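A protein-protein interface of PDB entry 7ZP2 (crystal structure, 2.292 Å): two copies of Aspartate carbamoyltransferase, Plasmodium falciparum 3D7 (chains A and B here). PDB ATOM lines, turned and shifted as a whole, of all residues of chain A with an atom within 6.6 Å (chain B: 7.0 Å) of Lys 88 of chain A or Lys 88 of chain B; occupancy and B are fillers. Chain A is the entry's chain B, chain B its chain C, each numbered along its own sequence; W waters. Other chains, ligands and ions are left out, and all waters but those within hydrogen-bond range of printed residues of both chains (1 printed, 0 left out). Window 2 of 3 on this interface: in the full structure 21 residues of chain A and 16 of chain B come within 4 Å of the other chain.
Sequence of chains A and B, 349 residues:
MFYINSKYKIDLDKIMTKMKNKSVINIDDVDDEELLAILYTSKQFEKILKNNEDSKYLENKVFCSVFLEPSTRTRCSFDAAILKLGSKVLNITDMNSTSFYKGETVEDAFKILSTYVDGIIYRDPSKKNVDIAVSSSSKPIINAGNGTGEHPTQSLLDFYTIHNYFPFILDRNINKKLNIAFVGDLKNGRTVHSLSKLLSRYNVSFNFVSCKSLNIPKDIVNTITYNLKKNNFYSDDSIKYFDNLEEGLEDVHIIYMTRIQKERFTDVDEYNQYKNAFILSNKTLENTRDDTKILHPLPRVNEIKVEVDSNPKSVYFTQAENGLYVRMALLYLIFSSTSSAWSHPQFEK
O of Ser 87 of chain A sits at hydrogen-bond distance from NZ of Lys 88 of chain B (3.3 Å).
The backbone carbonyl oxygen of Leu 58 of chain A sits at hydrogen-bond distance from the side-chain hydroxyl of Ser 87 of chain A (2.5 Å). The backbone NH (N) of Lys 61 of chain A lies within hydrogen-bond range of the side-chain hydroxyl (OG) of Ser 87 of chain A. The backbone carbonyl oxygen (O) of Lys 61 of chain A is in hydrogen-bond range of the backbone NH (N) of Lys 88 of chain A, at 2.8 Å. The backbone carbonyl oxygen (O) of Lys 88 of chain A sits at hydrogen-bond distance from the backbone NH (N) of Phe 63 of chain A (2.9 Å). The backbone carbonyl oxygen of Ile 82 of chain A lies within hydrogen-bond range of the backbone NH of Ser 87 of chain A, 3.1 Å away. O of Phe 63 of chain B lies within hydrogen-bond range of N of Leu 90 of chain B, 2.9 Å away.
Among the printed residues, merely in contact across the chains: Lys 56 of chain A with Asn 60 of chain B (3.4 Å), Leu 83 of chain A with Lys 88 of chain B (3.5 Å), Leu 83 of chain A with Val 89 of chain B (3.8 Å), Leu 83 of chain A with Leu 90 of chain B (3.97 Å), Lys 84 of chain A with Val 62 of chain B (3.7 Å) and Lys 88 of chain A with Lys 88 of chain B (3.9 Å).
Lys 88 of chain B touches just these residues of chain A: Leu 83 (3.5 Å), Ser 87 (3.3 Å) and Lys 88 (3.9 Å). Of the printed residues of chain A, Val 62 of chain B touches Lys 84. Of the printed residues of chain B, Lys 84 of chain A touches Val 62. The nearest residue of chain A that does not touch Lys 88 of chain B is Lys 56 of chain A (4.03 Å).
Of the 16 printed residues of chain B, 5 touch a printed residue of chain A. Printed residues of chain B that touch a printed residue of chain A: Asn 60, Val 62, Lys 88, Val 89 and Leu 90. Along chain B the printed residues that touch a printed residue of chain A span positions 60 to 90. Hydrophobic or aromatic side chains of chain A that line the printed part of chain B: Leu 83. Among the printed residues, 7 pairs touch across the chains. Among the printed residues, no Asp or Glu carboxylate lies within 4 Å of a Lys or Arg side-chain nitrogen of the other chain.
Lys 56 of chain A touches Asn 60 of chain B, but with the chains exchanged Asn 60 of chain A does not touch Lys 56 of chain B (11.2 Å). Leu 83 of chain A touches Val 89 of chain B, but with the chains exchanged Val 89 of chain A does not touch Leu 83 of chain B (9.1 Å). Leu 83 of chain A touches Leu 90 of chain B, but with the chains exchanged Leu 90 of chain A does not touch Leu 83 of chain B (11.3 Å). Lys 88 of chain A touches its own counterpart, Lys 88 of chain B. Positions printed for both chains: 56, 58, 59, 60, 61, 62, 63, 64, 82, 83, 86, 87, 88, 89 and 90. Of the 7 pairs that touch across the chains among the printed residues, 1 has its exchanged pair printed and touching as well.
Water W1 lies within hydrogen-bond range of O of Asn 60 of chain B (2.8 Å) and NZ of Lys 84 of chain A (2.9 Å).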
ATOM      1  N   LYS A  56       4.062  -0.663  32.079  1.00  0.00           N
ATOM      2  CA  LYS A  56       5.005  -1.610  31.468  1.00  0.00           C
ATOM      3  C   LYS A  56       5.714  -2.460  32.524  1.00  0.00           C
ATOM      4  O   LYS A  56       6.942  -2.468  32.555  1.00  0.00           O
ATOM      5  CB  LYS A  56       5.959  -0.848  30.545  1.00  0.00           C
ATOM      6  CG  LYS A  56       5.301  -0.284  29.278  1.00  0.00           C
ATOM      7  CD  LYS A  56       6.324   0.105  28.206  1.00  0.00           C
ATOM      8  CE  LYS A  56       5.696   0.688  26.954  1.00  0.00           C
ATOM      9  NZ  LYS A  56       6.294   0.189  25.664  1.00  0.00           N
ATOM     10  N   LEU A  58       5.810  -5.848  32.311  1.00  0.00           N
ATOM     11  CA  LEU A  58       6.251  -7.118  31.655  1.00  0.00           C
ATOM     12  C   LEU A  58       6.592  -6.844  30.190  1.00  0.00           C
ATOM     13  O   LEU A  58       5.764  -7.110  29.320  1.00  0.00           O
ATOM     14  CB  LEU A  58       5.138  -8.185  31.771  1.00  0.00           C
ATOM     15  CG  LEU A  58       5.562  -9.577  31.358  1.00  0.00           C
ATOM     16  CD1 LEU A  58       6.540 -10.200  32.387  1.00  0.00           C
ATOM     17  CD2 LEU A  58       4.326 -10.424  31.114  1.00  0.00           C
ATOM     18  N   GLU A  59       7.868  -6.587  29.912  1.00  0.00           N
ATOM     19  CA  GLU A  59       8.377  -5.997  28.667  1.00  0.00           C
ATOM     20  C   GLU A  59       9.034  -6.969  27.686  1.00  0.00           C
ATOM     21  O   GLU A  59       9.012  -6.662  26.489  1.00  0.00           O
ATOM     22  CB  GLU A  59       9.394  -4.914  29.018  1.00  0.00           C
ATOM     23  CG  GLU A  59       8.737  -3.664  29.557  1.00  0.00           C
ATOM     24  CD  GLU A  59       9.644  -2.450  29.624  1.00  0.00           C
ATOM     25  OE1 GLU A  59      10.505  -2.396  30.568  1.00  0.00           O
ATOM     26  OE2 GLU A  59       9.474  -1.589  28.747  1.00  0.00           O
ATOM     27  N   ASN A  60       9.656  -8.039  28.062  1.00  0.00           N
ATOM     28  CA  ASN A  60      10.488  -8.670  26.992  1.00  0.00           C
ATOM     29  C   ASN A  60       9.833  -9.929  26.432  1.00  0.00           C
ATOM     30  O   ASN A  60      10.523 -10.798  25.988  1.00  0.00           O
ATOM     31  CB  ASN A  60      11.866  -8.912  27.572  1.00  0.00           C
ATOM     32  CG  ASN A  60      12.352  -7.607  28.145  1.00  0.00           C
ATOM     33  OD1 ASN A  60      12.611  -6.653  27.395  1.00  0.00           O
ATOM     34  ND2 ASN A  60      12.448  -7.590  29.465  1.00  0.00           N
ATOM     35  N   LYS A  61       8.548 -10.071  26.632  1.00  0.00           N
ATOM     36  CA  LYS A  61       7.839 -11.328  26.263  1.00  0.00           C
ATOM     37  C   LYS A  61       7.206 -11.217  24.880  1.00  0.00           C
ATOM     38  O   LYS A  61       6.737 -10.085  24.471  1.00  0.00           O
ATOM     39  CB  LYS A  61       6.766 -11.638  27.310  1.00  0.00           C
ATOM     40  CG  LYS A  61       7.309 -11.783  28.710  1.00  0.00           C
ATOM     41  CD  LYS A  61       8.413 -12.878  28.790  1.00  0.00           C
ATOM     42  CE  LYS A  61       9.287 -12.755  30.006  1.00  0.00           C
ATOM     43  NZ  LYS A  61       9.415 -14.068  30.696  1.00  0.00           N
ATOM     44  N   VAL A  62       7.133 -12.367  24.225  1.00  0.00           N
ATOM     45  CA  VAL A  62       6.423 -12.545  22.932  1.00  0.00           C
ATOM     46  C   VAL A  62       5.421 -13.675  23.148  1.00  0.00           C
ATOM     47  O   VAL A  62       5.826 -14.766  23.552  1.00  0.00           O
ATOM     48  CB  VAL A  62       7.401 -12.848  21.796  1.00  0.00           C
ATOM     49  CG1 VAL A  62       6.650 -13.113  20.499  1.00  0.00           C
ATOM     50  CG2 VAL A  62       8.362 -11.647  21.638  1.00  0.00           C
ATOM     51  N   PHE A  63       4.160 -13.367  22.908  1.00  0.00           N
ATOM     52  CA  PHE A  63       3.056 -14.338  23.028  1.00  0.00           C
ATOM     53  C   PHE A  63       2.559 -14.670  21.639  1.00  0.00           C
ATOM     54  O   PHE A  63       2.754 -13.868  20.686  1.00  0.00           O
ATOM     55  CB  PHE A  63       1.949 -13.727  23.876  1.00  0.00           C
ATOM     56  CG  PHE A  63       2.329 -13.419  25.299  1.00  0.00           C
ATOM     57  CD1 PHE A  63       2.777 -12.167  25.656  1.00  0.00           C
ATOM     58  CD2 PHE A  63       2.196 -14.352  26.305  1.00  0.00           C
ATOM     59  CE1 PHE A  63       3.099 -11.860  26.971  1.00  0.00           C
ATOM     60  CE2 PHE A  63       2.407 -14.014  27.646  1.00  0.00           C
ATOM     61  CZ  PHE A  63       2.887 -12.769  27.982  1.00  0.00           C
ATOM     62  N   CYS A  64       1.877 -15.788  21.551  1.00  0.00           N
ATOM     63  CA  CYS A  64       0.988 -16.112  20.423  1.00  0.00           C
ATOM     64  C   CYS A  64      -0.446 -16.146  20.983  1.00  0.00           C
ATOM     65  O   CYS A  64      -0.698 -16.747  22.018  1.00  0.00           O
ATOM     66  CB  CYS A  64       1.357 -17.425  19.767  1.00  0.00           C
ATOM     67  SG  CYS A  64       0.257 -17.787  18.357  1.00  0.00           S
ATOM     68  N   ILE A  82      -1.482  -7.450  26.913  1.00  0.00           N
ATOM     69  CA  ILE A  82      -0.078  -7.785  26.564  1.00  0.00           C
ATOM     70  C   ILE A  82       0.623  -6.506  26.170  1.00  0.00           C
ATOM     71  O   ILE A  82       1.779  -6.309  26.608  1.00  0.00           O
ATOM     72  CB  ILE A  82      -0.039  -8.807  25.427  1.00  0.00           C
ATOM     73  CG1 ILE A  82      -0.573 -10.149  25.901  1.00  0.00           C
ATOM     74  CG2 ILE A  82       1.357  -8.914  24.875  1.00  0.00           C
ATOM     75  CD1 ILE A  82      -0.996 -11.006  24.755  1.00  0.00           C
ATOM     76  N   LEU A  83      -0.004  -5.728  25.287  1.00  0.00           N
ATOM     77  CA  LEU A  83       0.680  -4.556  24.714  1.00  0.00           C
ATOM     78  C   LEU A  83       0.881  -3.487  25.824  1.00  0.00           C
ATOM     79  O   LEU A  83       1.957  -2.915  25.897  1.00  0.00           O
ATOM     80  CB  LEU A  83      -0.117  -4.052  23.510  1.00  0.00           C
ATOM     81  CG  LEU A  83      -0.210  -5.022  22.331  1.00  0.00           C
ATOM     82  CD1 LEU A  83      -1.233  -4.514  21.338  1.00  0.00           C
ATOM     83  CD2 LEU A  83       1.141  -5.234  21.639  1.00  0.00           C
ATOM     84  N   LYS A  84      -0.068  -3.297  26.710  1.00  0.00           N
ATOM     85  CA  LYS A  84      -0.035  -2.270  27.800  1.00  0.00           C
ATOM     86  C   LYS A  84       1.056  -2.638  28.816  1.00  0.00           C
ATOM     87  O   LYS A  84       1.675  -1.680  29.382  1.00  0.00           O
ATOM     88  CB  LYS A  84      -1.380  -2.199  28.524  1.00  0.00           C
ATOM     89  CG  LYS A  84      -2.437  -1.271  27.952  1.00  0.00           C
ATOM     90  CD  LYS A  84      -1.983   0.214  27.904  1.00  0.00           C
ATOM     91  CE  LYS A  84      -2.015   0.995  29.207  1.00  0.00           C
ATOM     92  NZ  LYS A  84      -0.971   2.059  29.301  1.00  0.00           N
ATOM     93  N   GLY A  86       3.748  -4.054  27.931  1.00  0.00           N
ATOM     94  CA  GLY A  86       4.944  -3.670  27.167  1.00  0.00           C
ATOM     95  C   GLY A  86       5.554  -4.850  26.434  1.00  0.00           C
ATOM     96  O   GLY A  86       6.663  -4.699  25.942  1.00  0.00           O
ATOM     97  N   SER A  87       4.831  -5.970  26.348  1.00  0.00           N
ATOM     98  CA  SER A  87       5.264  -7.175  25.598  1.00  0.00           C
ATOM     99  C   SER A  87       4.675  -7.146  24.180  1.00  0.00           C
ATOM    100  O   SER A  87       4.098  -6.086  23.750  1.00  0.00           O
ATOM    101  CB  SER A  87       4.900  -8.413  26.421  1.00  0.00           C
ATOM    102  OG  SER A  87       5.937  -8.658  27.331  1.00  0.00           O
ATOM    103  N   LYS A  88       4.845  -8.238  23.450  1.00  0.00           N
ATOM    104  CA  LYS A  88       4.522  -8.289  21.993  1.00  0.00           C
ATOM    105  C   LYS A  88       3.732  -9.576  21.716  1.00  0.00           C
ATOM    106  O   LYS A  88       3.754 -10.517  22.587  1.00  0.00           O
ATOM    107  CB  LYS A  88       5.809  -8.327  21.208  1.00  0.00           C
ATOM    108  CG  LYS A  88       6.467  -6.961  21.029  1.00  0.00           C
ATOM    109  CD  LYS A  88       7.983  -7.230  20.738  1.00  0.00           C
ATOM    110  CE  LYS A  88       8.775  -5.960  20.802  1.00  0.00           C
ATOM    111  NZ  LYS A  88       8.162  -4.953  19.927  1.00  0.00           N
ATOM    112  N   VAL A  89       2.945  -9.561  20.664  1.00  0.00           N
ATOM    113  CA  VAL A  89       2.012 -10.687  20.385  1.00  0.00           C
ATOM    114  C   VAL A  89       1.847 -10.865  18.890  1.00  0.00           C
ATOM    115  O   VAL A  89       1.824  -9.918  18.145  1.00  0.00           O
ATOM    116  CB  VAL A  89       0.656 -10.573  21.108  1.00  0.00           C
ATOM    117  CG1 VAL A  89      -0.095  -9.306  20.745  1.00  0.00           C
ATOM    118  CG2 VAL A  89      -0.216 -11.813  20.797  1.00  0.00           C
ATOM    119  N   LEU A  90       1.919 -12.133  18.472  1.00  0.00           N
ATOM    120  CA  LEU A  90       1.515 -12.502  17.099  1.00  0.00           C
ATOM    121  C   LEU A  90       0.150 -13.213  17.191  1.00  0.00           C
ATOM    122  O   LEU A  90      -0.081 -14.010  18.172  1.00  0.00           O
ATOM    123  CB  LEU A  90       2.611 -13.354  16.424  1.00  0.00           C
ATOM    124  CG  LEU A  90       3.115 -14.595  17.182  1.00  0.00           C
ATOM    125  CD1 LEU A  90       3.288 -15.805  16.263  1.00  0.00           C
ATOM    126  CD2 LEU A  90       4.411 -14.314  17.918  1.00  0.00           C
ATOM    127  N   LYS B  56      10.683   7.822  17.175  1.00  0.00           N
ATOM    128  CA  LYS B  56       9.827   7.361  18.291  1.00  0.00           C
ATOM    129  C   LYS B  56       9.383   8.546  19.161  1.00  0.00           C
ATOM    130  O   LYS B  56       9.801   8.645  20.279  1.00  0.00           O
ATOM    131  CB  LYS B  56      10.604   6.315  19.078  1.00  0.00           C
ATOM    132  CG  LYS B  56      10.818   4.967  18.357  1.00  0.00           C
ATOM    133  CD  LYS B  56      11.254   3.820  19.304  1.00  0.00           C
ATOM    134  CE  LYS B  56      10.490   2.513  19.070  1.00  0.00           C
ATOM    135  NZ  LYS B  56      11.165   1.299  19.639  1.00  0.00           N
ATOM    136  N   LEU B  58       6.137   9.090  19.966  1.00  0.00           N
ATOM    137  CA  LEU B  58       4.853   8.756  20.635  1.00  0.00           C
ATOM    138  C   LEU B  58       4.928   7.277  21.008  1.00  0.00           C
ATOM    139  O   LEU B  58       4.357   6.432  20.348  1.00  0.00           O
ATOM    140  CB  LEU B  58       3.643   9.088  19.783  1.00  0.00           C
ATOM    141  CG  LEU B  58       2.300   8.888  20.459  1.00  0.00           C
ATOM    142  CD1 LEU B  58       2.015  10.023  21.452  1.00  0.00           C
ATOM    143  CD2 LEU B  58       1.204   8.744  19.416  1.00  0.00           C
ATOM    144  N   GLU B  59       5.656   7.060  22.084  1.00  0.00           N
ATOM    145  CA  GLU B  59       5.858   5.828  22.817  1.00  0.00           C
ATOM    146  C   GLU B  59       4.665   5.682  23.757  1.00  0.00           C
ATOM    147  O   GLU B  59       3.980   6.763  24.101  1.00  0.00           O
ATOM    148  CB  GLU B  59       7.215   5.991  23.512  1.00  0.00           C
ATOM    149  CG  GLU B  59       8.351   6.111  22.522  1.00  0.00           C
ATOM    150  CD  GLU B  59       9.761   6.300  23.086  1.00  0.00           C
ATOM    151  OE1 GLU B  59      10.174   7.435  23.597  1.00  0.00           O
ATOM    152  OE2 GLU B  59      10.507   5.377  22.882  1.00  0.00           O
ATOM    153  N   ASN B  60       4.382   4.443  24.145  1.00  0.00           N
ATOM    154  CA  ASN B  60       3.607   4.099  25.358  1.00  0.00           C
ATOM    155  C   ASN B  60       2.095   4.112  25.075  1.00  0.00           C
ATOM    156  O   ASN B  60       1.355   3.789  25.965  1.00  0.00           O
ATOM    157  CB  ASN B  60       3.899   5.014  26.547  1.00  0.00           C
ATOM    158  CG  ASN B  60       5.337   5.076  26.994  1.00  0.00           C
ATOM    159  OD1 ASN B  60       6.056   4.114  26.998  1.00  0.00           O
ATOM    160  ND2 ASN B  60       5.781   6.261  27.355  1.00  0.00           N
ATOM    161  N   LYS B  61       1.656   4.399  23.873  1.00  0.00           N
ATOM    162  CA  LYS B  61       0.239   4.296  23.497  1.00  0.00           C
ATOM    163  C   LYS B  61      -0.074   2.942  22.834  1.00  0.00           C
ATOM    164  O   LYS B  61       0.833   2.304  22.153  1.00  0.00           O
ATOM    165  CB  LYS B  61      -0.091   5.402  22.508  1.00  0.00           C
ATOM    166  CG  LYS B  61       0.157   6.796  23.028  1.00  0.00           C
ATOM    167  CD  LYS B  61      -0.589   7.080  24.357  1.00  0.00           C
ATOM    168  CE  LYS B  61       0.065   8.152  25.193  1.00  0.00           C
ATOM    169  NZ  LYS B  61      -0.483   8.064  26.590  1.00  0.00           N
ATOM    170  N   VAL B  62      -1.310   2.517  23.050  1.00  0.00           N
ATOM    171  CA  VAL B  62      -1.895   1.277  22.494  1.00  0.00           C
ATOM    172  C   VAL B  62      -3.165   1.679  21.775  1.00  0.00           C
ATOM    173  O   VAL B  62      -4.017   2.344  22.406  1.00  0.00           O
ATOM    174  CB  VAL B  62      -2.191   0.290  23.636  1.00  0.00           C
ATOM    175  CG1 VAL B  62      -2.841  -0.982  23.130  1.00  0.00           C
ATOM    176  CG2 VAL B  62      -0.907  -0.006  24.420  1.00  0.00           C
ATOM    177  N   PHE B  63      -3.246   1.378  20.490  1.00  0.00           N
ATOM    178  CA  PHE B  63      -4.372   1.796  19.626  1.00  0.00           C
ATOM    179  C   PHE B  63      -5.108   0.530  19.207  1.00  0.00           C
ATOM    180  O   PHE B  63      -4.541  -0.554  19.213  1.00  0.00           O
ATOM    181  CB  PHE B  63      -3.891   2.506  18.374  1.00  0.00           C
ATOM    182  CG  PHE B  63      -3.220   3.811  18.640  1.00  0.00           C
ATOM    183  CD1 PHE B  63      -1.868   3.912  18.786  1.00  0.00           C
ATOM    184  CD2 PHE B  63      -3.981   4.998  18.622  1.00  0.00           C
ATOM    185  CE1 PHE B  63      -1.292   5.164  19.072  1.00  0.00           C
ATOM    186  CE2 PHE B  63      -3.402   6.235  18.863  1.00  0.00           C
ATOM    187  CZ  PHE B  63      -2.046   6.314  19.100  1.00  0.00           C
ATOM    188  N   CYS B  64      -6.363   0.708  18.858  1.00  0.00           N
ATOM    189  CA  CYS B  64      -7.175  -0.285  18.149  1.00  0.00           C
ATOM    190  C   CYS B  64      -7.485   0.287  16.763  1.00  0.00           C
ATOM    191  O   CYS B  64      -7.873   1.448  16.644  1.00  0.00           O
ATOM    192  CB  CYS B  64      -8.438  -0.661  18.876  1.00  0.00           C
ATOM    193  SG  CYS B  64      -9.293  -2.011  18.049  1.00  0.00           S
ATOM    194  N   ILE B  82       1.843   4.291  13.450  1.00  0.00           N
ATOM    195  CA  ILE B  82       1.781   4.003  14.910  1.00  0.00           C
ATOM    196  C   ILE B  82       3.079   3.322  15.310  1.00  0.00           C
ATOM    197  O   ILE B  82       3.630   3.664  16.377  1.00  0.00           O
ATOM    198  CB  ILE B  82       0.592   3.098  15.236  1.00  0.00           C
ATOM    199  CG1 ILE B  82      -0.705   3.831  15.092  1.00  0.00           C
ATOM    200  CG2 ILE B  82       0.724   2.473  16.592  1.00  0.00           C
ATOM    201  CD1 ILE B  82      -1.880   2.886  14.880  1.00  0.00           C
ATOM    202  N   LEU B  83       3.491   2.332  14.533  1.00  0.00           N
ATOM    203  CA  LEU B  83       4.636   1.495  14.955  1.00  0.00           C
ATOM    204  C   LEU B  83       5.929   2.336  14.873  1.00  0.00           C
ATOM    205  O   LEU B  83       6.752   2.251  15.796  1.00  0.00           O
ATOM    206  CB  LEU B  83       4.637   0.211  14.129  1.00  0.00           C
ATOM    207  CG  LEU B  83       3.434  -0.702  14.334  1.00  0.00           C
ATOM    208  CD1 LEU B  83       3.466  -1.807  13.281  1.00  0.00           C
ATOM    209  CD2 LEU B  83       3.422  -1.323  15.738  1.00  0.00           C
ATOM    210  N   GLY B  86       6.502   4.464  17.740  1.00  0.00           N
ATOM    211  CA  GLY B  86       6.978   3.609  18.847  1.00  0.00           C
ATOM    212  C   GLY B  86       5.855   3.168  19.763  1.00  0.00           C
ATOM    213  O   GLY B  86       6.140   2.676  20.836  1.00  0.00           O
ATOM    214  N   SER B  87       4.607   3.331  19.332  1.00  0.00           N
ATOM    215  CA  SER B  87       3.395   2.841  20.002  1.00  0.00           C
ATOM    216  C   SER B  87       2.998   1.479  19.442  1.00  0.00           C
ATOM    217  O   SER B  87       3.830   0.842  18.705  1.00  0.00           O
ATOM    218  CB  SER B  87       2.307   3.912  19.904  1.00  0.00           C
ATOM    219  OG  SER B  87       2.517   4.857  20.959  1.00  0.00           O
ATOM    220  N   LYS B  88       1.843   0.971  19.855  1.00  0.00           N
ATOM    221  CA  LYS B  88       1.461  -0.451  19.636  1.00  0.00           C
ATOM    222  C   LYS B  88       0.025  -0.483  19.177  1.00  0.00           C
ATOM    223  O   LYS B  88      -0.693   0.534  19.424  1.00  0.00           O
ATOM    224  CB  LYS B  88       1.628  -1.251  20.919  1.00  0.00           C
ATOM    225  CG  LYS B  88       3.056  -1.749  21.184  1.00  0.00           C
ATOM    226  CD  LYS B  88       3.191  -2.134  22.689  1.00  0.00           C
ATOM    227  CE  LYS B  88       4.676  -2.319  22.963  1.00  0.00           C
ATOM    228  NZ  LYS B  88       5.146  -3.468  22.110  1.00  0.00           N
ATOM    229  N   VAL B  89      -0.366  -1.509  18.425  1.00  0.00           N
ATOM    230  CA  VAL B  89      -1.744  -1.534  17.859  1.00  0.00           C
ATOM    231  C   VAL B  89      -2.279  -2.959  17.834  1.00  0.00           C
ATOM    232  O   VAL B  89      -1.521  -3.954  17.568  1.00  0.00           O
ATOM    233  CB  VAL B  89      -1.800  -0.853  16.468  1.00  0.00           C
ATOM    234  CG1 VAL B  89      -0.861  -1.469  15.458  1.00  0.00           C
ATOM    235  CG2 VAL B  89      -3.207  -0.883  15.902  1.00  0.00           C
ATOM    236  N   LEU B  90      -3.549  -3.095  18.143  1.00  0.00           N
ATOM    237  CA  LEU B  90      -4.280  -4.355  17.831  1.00  0.00           C
ATOM    238  C   LEU B  90      -5.244  -4.018  16.661  1.00  0.00           C
ATOM    239  O   LEU B  90      -5.885  -2.875  16.667  1.00  0.00           O
ATOM    240  CB  LEU B  90      -5.022  -4.879  19.069  1.00  0.00           C
ATOM    241  CG  LEU B  90      -5.833  -3.857  19.881  1.00  0.00           C
ATOM    242  CD1 LEU B  90      -7.221  -4.342  20.299  1.00  0.00           C
ATOM    243  CD2 LEU B  90      -5.055  -3.461  21.107  1.00  0.00           C
ATOM    244  N   ASP B 118      -6.040   3.667  23.912  1.00  0.00           N
ATOM    245  CA  ASP B 118      -5.841   5.147  24.023  1.00  0.00           C
ATOM    246  C   ASP B 118      -6.536   5.847  22.870  1.00  0.00           C
ATOM    247  O   ASP B 118      -6.863   7.043  22.954  1.00  0.00           O
ATOM    248  CB  ASP B 118      -4.350   5.472  24.073  1.00  0.00           C
ATOM    249  CG  ASP B 118      -3.679   4.777  25.246  1.00  0.00           C
ATOM    250  OD1 ASP B 118      -4.274   4.737  26.398  1.00  0.00           O
ATOM    251  OD2 ASP B 118      -2.685   4.112  25.008  1.00  0.00           O
HETATM  252  O   HOH W   1       1.591   1.755  27.938  1.00  0.00           O
